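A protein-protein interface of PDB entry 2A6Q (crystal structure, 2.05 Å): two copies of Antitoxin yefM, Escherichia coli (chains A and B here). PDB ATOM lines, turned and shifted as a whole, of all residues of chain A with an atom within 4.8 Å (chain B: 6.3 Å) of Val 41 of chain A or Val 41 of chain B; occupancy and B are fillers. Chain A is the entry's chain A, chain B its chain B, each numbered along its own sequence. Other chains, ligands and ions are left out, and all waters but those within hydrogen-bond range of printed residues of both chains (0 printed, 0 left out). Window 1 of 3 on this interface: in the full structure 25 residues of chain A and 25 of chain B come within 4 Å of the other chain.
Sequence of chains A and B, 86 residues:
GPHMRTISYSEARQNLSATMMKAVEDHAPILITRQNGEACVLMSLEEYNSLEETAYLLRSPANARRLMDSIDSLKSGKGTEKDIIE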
ATOM      1  N   MET A   4      -6.238  17.716  14.197  1.00  0.00           N
ATOM      2  CA  MET A   4      -6.134  16.283  13.999  1.00  0.00           C
ATOM      3  C   MET A   4      -5.544  15.948  12.649  1.00  0.00           C
ATOM      4  O   MET A   4      -5.506  16.772  11.727  1.00  0.00           O
ATOM      5  CB  MET A   4      -7.512  15.606  14.143  1.00  0.00           C
ATOM      6  CG  MET A   4      -8.510  15.932  13.050  1.00  0.00           C
ATOM      7  SD  MET A   4     -10.060  14.966  13.200  1.00  0.00           S
ATOM      8  CE  MET A   4     -10.766  15.721  14.678  1.00  0.00           C
ATOM      9  N   PRO A  29      -8.721  10.435  16.394  1.00  0.00           N
ATOM     10  CA  PRO A  29      -9.631  10.715  15.278  1.00  0.00           C
ATOM     11  C   PRO A  29      -8.874  11.150  14.029  1.00  0.00           C
ATOM     12  O   PRO A  29      -7.729  11.586  14.112  1.00  0.00           O
ATOM     13  CB  PRO A  29     -10.500  11.834  15.832  1.00  0.00           C
ATOM     14  CG  PRO A  29      -9.502  12.631  16.632  1.00  0.00           C
ATOM     15  CD  PRO A  29      -8.713  11.553  17.360  1.00  0.00           C
ATOM     16  N   ILE A  30      -9.497  11.012  12.865  1.00  0.00           N
ATOM     17  CA  ILE A  30      -8.849  11.464  11.648  1.00  0.00           C
ATOM     18  C   ILE A  30      -9.885  12.187  10.788  1.00  0.00           C
ATOM     19  O   ILE A  30     -11.054  11.790  10.732  1.00  0.00           O
ATOM     20  CB  ILE A  30      -8.175  10.296  10.876  1.00  0.00           C
ATOM     21  CG1 ILE A  30      -7.317  10.859   9.735  1.00  0.00           C
ATOM     22  CG2 ILE A  30      -9.218   9.340  10.330  1.00  0.00           C
ATOM     23  CD1 ILE A  30      -6.398   9.836   9.053  1.00  0.00           C
ATOM     24  N   LEU A  31      -9.462  13.271  10.146  1.00  0.00           N
ATOM     25  CA  LEU A  31     -10.367  14.067   9.313  1.00  0.00           C
ATOM     26  C   LEU A  31     -10.226  13.704   7.840  1.00  0.00           C
ATOM     27  O   LEU A  31      -9.146  13.836   7.259  1.00  0.00           O
ATOM     28  CB  LEU A  31     -10.075  15.560   9.486  1.00  0.00           C
ATOM     29  CG  LEU A  31     -10.943  16.546   8.685  1.00  0.00           C
ATOM     30  CD1 LEU A  31     -12.355  16.563   9.265  1.00  0.00           C
ATOM     31  CD2 LEU A  31     -10.341  17.937   8.755  1.00  0.00           C
ATOM     32  N   ALA A  39     -16.160  17.351   4.634  1.00  0.00           N
ATOM     33  CA  ALA A  39     -15.200  16.755   5.558  1.00  0.00           C
ATOM     34  C   ALA A  39     -15.858  16.137   6.786  1.00  0.00           C
ATOM     35  O   ALA A  39     -16.671  16.772   7.474  1.00  0.00           O
ATOM     36  CB  ALA A  39     -14.177  17.795   5.992  1.00  0.00           C
ATOM     37  N   CYS A  40     -15.488  14.890   7.058  1.00  0.00           N
ATOM     38  CA  CYS A  40     -16.007  14.158   8.199  1.00  0.00           C
ATOM     39  C   CYS A  40     -14.882  13.569   9.017  1.00  0.00           C
ATOM     40  O   CYS A  40     -13.840  13.203   8.483  1.00  0.00           O
ATOM     41  CB  CYS A  40     -16.898  13.010   7.748  1.00  0.00           C
ATOM     42  SG  CYS A  40     -18.351  13.524   6.918  1.00  0.00           S
ATOM     43  N   VAL A  41     -15.113  13.472  10.317  1.00  0.00           N
ATOM     44  CA  VAL A  41     -14.150  12.891  11.224  1.00  0.00           C
ATOM     45  C   VAL A  41     -14.521  11.420  11.376  1.00  0.00           C
ATOM     46  O   VAL A  41     -15.706  11.059  11.426  1.00  0.00           O
ATOM     47  CB  VAL A  41     -14.203  13.576  12.617  1.00  0.00           C
ATOM     48  CG1 VAL A  41     -13.237  12.886  13.582  1.00  0.00           C
ATOM     49  CG2 VAL A  41     -13.853  15.063  12.485  1.00  0.00           C
ATOM     50  N   LEU A  42     -13.505  10.568  11.399  1.00  0.00           N
ATOM     51  CA  LEU A  42     -13.695   9.142  11.600  1.00  0.00           C
ATOM     52  C   LEU A  42     -12.997   8.826  12.917  1.00  0.00           C
ATOM     53  O   LEU A  42     -11.862   9.255  13.137  1.00  0.00           O
ATOM     54  CB  LEU A  42     -13.034   8.336  10.476  1.00  0.00           C
ATOM     55  CG  LEU A  42     -12.998   6.819  10.701  1.00  0.00           C
ATOM     56  CD1 LEU A  42     -14.373   6.239  10.414  1.00  0.00           C
ATOM     57  CD2 LEU A  42     -11.962   6.177   9.794  1.00  0.00           C
ATOM     58  N   MET A  43     -13.673   8.109  13.807  1.00  0.00           N
ATOM     59  CA  MET A  43     -13.059   7.742  15.076  1.00  0.00           C
ATOM     60  C   MET A  43     -13.572   6.378  15.482  1.00  0.00           C
ATOM     61  O   MET A  43     -14.608   5.928  14.987  1.00  0.00           O
ATOM     62  CB  MET A  43     -13.383   8.775  16.164  1.00  0.00           C
ATOM     63  CG  MET A  43     -14.865   8.912  16.510  1.00  0.00           C
ATOM     64  SD  MET A  43     -15.142  10.184  17.776  1.00  0.00           S
ATOM     65  CE  MET A  43     -15.320  11.594  16.824  1.00  0.00           C
ATOM     66  N   SER A  44     -12.847   5.716  16.376  1.00  0.00           N
ATOM     67  CA  SER A  44     -13.259   4.399  16.844  1.00  0.00           C
ATOM     68  C   SER A  44     -14.566   4.530  17.635  1.00  0.00           C
ATOM     69  O   SER A  44     -14.849   5.587  18.208  1.00  0.00           O
ATOM     70  CB  SER A  44     -12.171   3.791  17.731  1.00  0.00           C
ATOM     71  OG  SER A  44     -12.095   4.466  18.973  1.00  0.00           O
ATOM     72  N   LEU A  45     -15.364   3.464  17.657  1.00  0.00           N
ATOM     73  CA  LEU A  45     -16.629   3.489  18.389  1.00  0.00           C
ATOM     74  C   LEU A  45     -16.360   3.795  19.857  1.00  0.00           C
ATOM     75  O   LEU A  45     -17.089   4.548  20.499  1.00  0.00           O
ATOM     76  CB  LEU A  45     -17.345   2.138  18.280  1.00  0.00           C
ATOM     77  CG  LEU A  45     -18.665   2.035  19.059  1.00  0.00           C
ATOM     78  CD1 LEU A  45     -19.628   3.143  18.634  1.00  0.00           C
ATOM     79  CD2 LEU A  45     -19.280   0.662  18.813  1.00  0.00           C
ATOM     80  N   TYR A  48     -15.709   7.385  20.340  1.00  0.00           N
ATOM     81  CA  TYR A  48     -16.947   8.124  20.163  1.00  0.00           C
ATOM     82  C   TYR A  48     -17.822   8.017  21.416  1.00  0.00           C
ATOM     83  O   TYR A  48     -18.325   9.016  21.914  1.00  0.00           O
ATOM     84  CB  TYR A  48     -17.735   7.604  18.957  1.00  0.00           C
ATOM     85  CG  TYR A  48     -19.097   8.243  18.862  1.00  0.00           C
ATOM     86  CD1 TYR A  48     -19.237   9.571  18.464  1.00  0.00           C
ATOM     87  CD2 TYR A  48     -20.237   7.553  19.270  1.00  0.00           C
ATOM     88  CE1 TYR A  48     -20.479  10.203  18.485  1.00  0.00           C
ATOM     89  CE2 TYR A  48     -21.488   8.177  19.293  1.00  0.00           C
ATOM     90  CZ  TYR A  48     -21.598   9.501  18.903  1.00  0.00           C
ATOM     91  OH  TYR A  48     -22.818  10.132  18.967  1.00  0.00           O
ATOM     92  N   PRO B  29     -24.239  10.947  13.542  1.00  0.00           N
ATOM     93  CA  PRO B  29     -23.175   9.981  13.260  1.00  0.00           C
ATOM     94  C   PRO B  29     -23.631   8.661  12.639  1.00  0.00           C
ATOM     95  O   PRO B  29     -24.730   8.166  12.905  1.00  0.00           O
ATOM     96  CB  PRO B  29     -22.525   9.782  14.627  1.00  0.00           C
ATOM     97  CG  PRO B  29     -23.688   9.929  15.562  1.00  0.00           C
ATOM     98  CD  PRO B  29     -24.422  11.123  14.995  1.00  0.00           C
ATOM     99  N   ILE B  30     -22.769   8.105  11.800  1.00  0.00           N
ATOM    100  CA  ILE B  30     -23.034   6.838  11.146  1.00  0.00           C
ATOM    101  C   ILE B  30     -21.987   5.845  11.609  1.00  0.00           C
ATOM    102  O   ILE B  30     -20.783   6.131  11.599  1.00  0.00           O
ATOM    103  CB  ILE B  30     -22.971   6.969   9.611  1.00  0.00           C
ATOM    104  CG1 ILE B  30     -24.126   7.847   9.124  1.00  0.00           C
ATOM    105  CG2 ILE B  30     -23.036   5.597   8.975  1.00  0.00           C
ATOM    106  CD1 ILE B  30     -24.056   8.203   7.657  1.00  0.00           C
ATOM    107  N   LEU B  31     -22.454   4.678  12.029  1.00  0.00           N
ATOM    108  CA  LEU B  31     -21.577   3.625  12.506  1.00  0.00           C
ATOM    109  C   LEU B  31     -21.130   2.709  11.374  1.00  0.00           C
ATOM    110  O   LEU B  31     -21.960   2.179  10.633  1.00  0.00           O
ATOM    111  CB  LEU B  31     -22.297   2.788  13.565  1.00  0.00           C
ATOM    112  CG  LEU B  31     -21.545   1.565  14.094  1.00  0.00           C
ATOM    113  CD1 LEU B  31     -20.396   2.019  14.999  1.00  0.00           C
ATOM    114  CD2 LEU B  31     -22.514   0.668  14.866  1.00  0.00           C
ATOM    115  N   ILE B  32     -19.819   2.520  11.246  1.00  0.00           N
ATOM    116  CA  ILE B  32     -19.288   1.630  10.229  1.00  0.00           C
ATOM    117  C   ILE B  32     -18.853   0.360  10.947  1.00  0.00           C
ATOM    118  O   ILE B  32     -17.840   0.338  11.638  1.00  0.00           O
ATOM    119  CB  ILE B  32     -18.077   2.234   9.497  1.00  0.00           C
ATOM    120  CG1 ILE B  32     -18.470   3.554   8.833  1.00  0.00           C
ATOM    121  CG2 ILE B  32     -17.567   1.236   8.456  1.00  0.00           C
ATOM    122  CD1 ILE B  32     -17.316   4.260   8.107  1.00  0.00           C
ATOM    123  N   ALA B  39     -15.619  -1.455  15.138  1.00  0.00           N
ATOM    124  CA  ALA B  39     -16.369  -0.482  14.361  1.00  0.00           C
ATOM    125  C   ALA B  39     -15.860   0.935  14.586  1.00  0.00           C
ATOM    126  O   ALA B  39     -15.212   1.231  15.586  1.00  0.00           O
ATOM    127  CB  ALA B  39     -17.852  -0.567  14.724  1.00  0.00           C
ATOM    128  N   CYS B  40     -16.162   1.811  13.637  1.00  0.00           N
ATOM    129  CA  CYS B  40     -15.778   3.206  13.731  1.00  0.00           C
ATOM    130  C   CYS B  40     -17.010   4.056  13.494  1.00  0.00           C
ATOM    131  O   CYS B  40     -18.019   3.581  12.966  1.00  0.00           O
ATOM    132  CB  CYS B  40     -14.706   3.550  12.690  1.00  0.00           C
ATOM    133  SG  CYS B  40     -13.059   2.963  13.145  1.00  0.00           S
ATOM    134  N   VAL B  41     -16.928   5.315  13.890  1.00  0.00           N
ATOM    135  CA  VAL B  41     -18.026   6.244  13.695  1.00  0.00           C
ATOM    136  C   VAL B  41     -17.559   7.364  12.784  1.00  0.00           C
ATOM    137  O   VAL B  41     -16.415   7.820  12.881  1.00  0.00           O
ATOM    138  CB  VAL B  41     -18.489   6.845  15.045  1.00  0.00           C
ATOM    139  CG1 VAL B  41     -19.568   7.897  14.820  1.00  0.00           C
ATOM    140  CG2 VAL B  41     -19.011   5.730  15.944  1.00  0.00           C
ATOM    141  N   LEU B  42     -18.444   7.782  11.886  1.00  0.00           N
ATOM    142  CA  LEU B  42     -18.181   8.870  10.958  1.00  0.00           C
ATOM    143  C   LEU B  42     -19.185   9.970  11.289  1.00  0.00           C
ATOM    144  O   LEU B  42     -20.381   9.699  11.457  1.00  0.00           O
ATOM    145  CB  LEU B  42     -18.390   8.406   9.512  1.00  0.00           C
ATOM    146  CG  LEU B  42     -17.942   9.368   8.407  1.00  0.00           C
ATOM    147  CD1 LEU B  42     -16.415   9.442   8.390  1.00  0.00           C
ATOM    148  CD2 LEU B  42     -18.456   8.887   7.054  1.00  0.00           C
ATOM    149  N   MET B  43     -18.708  11.205  11.398  1.00  0.00           N
ATOM    150  CA  MET B  43     -19.592  12.319  11.708  1.00  0.00           C
ATOM    151  C   MET B  43     -19.012  13.574  11.097  1.00  0.00           C
ATOM    152  O   MET B  43     -17.819  13.617  10.780  1.00  0.00           O
ATOM    153  CB  MET B  43     -19.717  12.490  13.220  1.00  0.00           C
ATOM    154  CG  MET B  43     -18.444  12.985  13.901  1.00  0.00           C
ATOM    155  SD  MET B  43     -18.503  12.806  15.703  1.00  0.00           S
ATOM    156  CE  MET B  43     -19.728  13.938  16.095  1.00  0.00           C
ATOM    157  N   SER B  44     -19.846  14.595  10.927  1.00  0.00           N
ATOM    158  CA  SER B  44     -19.382  15.851  10.347  1.00  0.00           C
ATOM    159  C   SER B  44     -18.385  16.500  11.294  1.00  0.00           C
ATOM    160  O   SER B  44     -18.430  16.274  12.505  1.00  0.00           O
ATOM    161  CB  SER B  44     -20.556  16.812  10.129  1.00  0.00           C
ATOM    162  OG  SER B  44     -21.099  17.234  11.374  1.00  0.00           O
ATOM    163  N   LEU B  45     -17.492  17.311  10.739  1.00  0.00           N
ATOM    164  CA  LEU B  45     -16.506  18.011  11.551  1.00  0.00           C
ATOM    165  C   LEU B  45     -17.258  18.931  12.511  1.00  0.00           C
ATOM    166  O   LEU B  45     -16.897  19.069  13.680  1.00  0.00           O
ATOM    167  CB  LEU B  45     -15.583  18.840  10.654  1.00  0.00           C
ATOM    168  CG  LEU B  45     -14.602  19.771  11.368  1.00  0.00           C
ATOM    169  CD1 LEU B  45     -13.755  18.979  12.353  1.00  0.00           C
ATOM    170  CD2 LEU B  45     -13.737  20.470  10.336  1.00  0.00           C
ATOM    171  N   TYR B  48     -18.499  17.060  15.345  1.00  0.00           N
ATOM    172  CA  TYR B  48     -17.370  16.663  16.177  1.00  0.00           C
ATOM    173  C   TYR B  48     -16.876  17.801  17.080  1.00  0.00           C
ATOM    174  O   TYR B  48     -16.601  17.582  18.258  1.00  0.00           O
ATOM    175  CB  TYR B  48     -16.202  16.184  15.313  1.00  0.00           C
ATOM    176  CG  TYR B  48     -14.962  15.911  16.126  1.00  0.00           C
ATOM    177  CD1 TYR B  48     -14.814  14.715  16.813  1.00  0.00           C
ATOM    178  CD2 TYR B  48     -13.952  16.862  16.237  1.00  0.00           C
ATOM    179  CE1 TYR B  48     -13.689  14.466  17.591  1.00  0.00           C
ATOM    180  CE2 TYR B  48     -12.822  16.624  17.015  1.00  0.00           C
ATOM    181  CZ  TYR B  48     -12.702  15.421  17.685  1.00  0.00           C
ATOM    182  OH  TYR B  48     -11.581  15.153  18.432  1.00  0.00           O
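N of Val 41 of chain B sits at hydrogen-bond distance from O of Met 43 of chain A.
O of Ala 39 of chain B is in hydrogen-bond range of N of Leu 45 of chain A (3.0 Å).
O of Met 43 of chain B sits at hydrogen-bond distance from N of Val 41 of chain A, at 2.7 Å.
The backbone NH (N) of Leu 45 of chain B is in hydrogen-bond range of the backbone carbonyl oxygen (O) of Ala 39 of chain A (3.4 Å).
The backbone NH (N) of Leu 42 of chain A lies within hydrogen-bond range of the backbone carbonyl oxygen (O) of Ile 30 of chain A (2.8 Å).
The backbone NH (N) of Leu 42 of chain B is in hydrogen-bond range of the backbone carbonyl oxygen (O) of Ile 30 of chain B, at 2.9 Å.
The side-chain sulfur of Met 4 of chain A is in hydrogen-bond range of the backbone NH of Leu 31 of chain A, 3.5 Å away.
The backbone NH (N) of Ile 32 of chain B sits at hydrogen-bond distance from the backbone carbonyl oxygen (O) of Cys 40 of chain B (2.7 Å).
Among the printed residues, merely in contact across the chains: Met 43 of chain A with Tyr 48 of chain B (3.2 Å), Cys 40 of chain A with Met 43 of chain B (3.2 Å), Met 43 of chain A with Cys 40 of chain B (3.2 Å), Met 4 of chain A with Tyr 48 of chain B (3.2 Å), Leu 42 of chain A with Val 41 of chain B (3.3 Å), Val 41 of chain A with Leu 42 of chain B (3.3 Å), Tyr 48 of chain A with Pro 29 of chain B (3.5 Å), Leu 42 of chain A with Cys 40 of chain B (3.5 Å), Met 43 of chain A with Met 43 of chain B (3.6 Å), Val 41 of chain A with Val 41 of chain B (3.6 Å), Cys 40 of chain A with Leu 42 of chain B (3.7 Å), Pro 29 of chain A with Tyr 48 of chain B (3.7 Å), Tyr 48 of chain A with Val 41 of chain B (3.8 Å), Leu 45 of chain A with Val 41 of chain B (3.8 Å), Val 41 of chain A with Tyr 48 of chain B (3.8 Å), Leu 45 of chain A with Leu 31 of chain B (3.9 Å), Val 41 of chain A with Leu 45 of chain B (3.9 Å), Ser 44 of chain A with Ala 39 of chain B (3.9 Å), Leu 45 of chain A with Cys 40 of chain B (3.96 Å) and Ser 44 of chain A with Cys 40 of chain B (3.97 Å).
Ile 30 of chain A touches none of the printed residues of chain B.
Printed residues of chain B within 4 Å of Cys 40 of chain A: Leu 42 and Met 43.
Printed residues of chain B within 4 Å of Met 43 of chain A: Cys 40, Val 41, Met 43 and Tyr 48.
Ile 30 of chain B touches none of the printed residues of chain A.
Printed residues of chain A within 4 Å of Leu 31 of chain B: Leu 45.
Of chain A, only Val 41, Leu 42, Met 43, Leu 45 and Tyr 48 come within 4 Å of Val 41 of chain B.
Printed residues of chain A within 4 Å of Tyr 48 of chain B: Met 4 (3.2 Å), Pro 29 (3.7 Å), Val 41 (3.8 Å) and Met 43 (3.2 Å).
The nearest residue of chain A that does not touch Val 41 of chain B is Ser 44 of chain A (4.5 Å).
The nearest printed residue of chain B that does not touch Pro 29 of chain A is Val 41 of chain B (7.7 Å).
Of the 12 printed residues of chain B, 9 touch a printed residue of chain A.
Along chain B the printed residues that touch a printed residue of chain A span positions 29 to 48.
Of the 12 printed residues of chain A, 10 touch a printed residue of chain B.
Hydrophobic or aromatic side chains of chain A within 4 Å of the printed part of chain B: Met 4, Pro 29, Val 41, Leu 42, Met 43, Leu 45 and Tyr 48.
Among the printed residues, no Asp or Glu carboxylate lies within 4 Å of a Lys or Arg side-chain nitrogen of the other chain.
Pro 29 of chain A touches Tyr 48 of chain B, and with the chains exchanged Tyr 48 of chain A touches Pro 29 of chain B.
Met 43 of chain A touches Tyr 48 of chain B, but with the chains exchanged Tyr 48 of chain A does not touch Met 43 of chain B (4.3 Å).
Ser 44 of chain A touches Ala 39 of chain B, but with the chains exchanged Ala 39 of chain A does not touch Ser 44 of chain B (4.1 Å).
Leu 45 of chain A touches Cys 40 of chain B, but with the chains exchanged Cys 40 of chain A does not touch Leu 45 of chain B (4.3 Å).
Of the 24 pairs that touch across the chains among the printed residues, 18 have their exchanged pair printed and touching as well.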
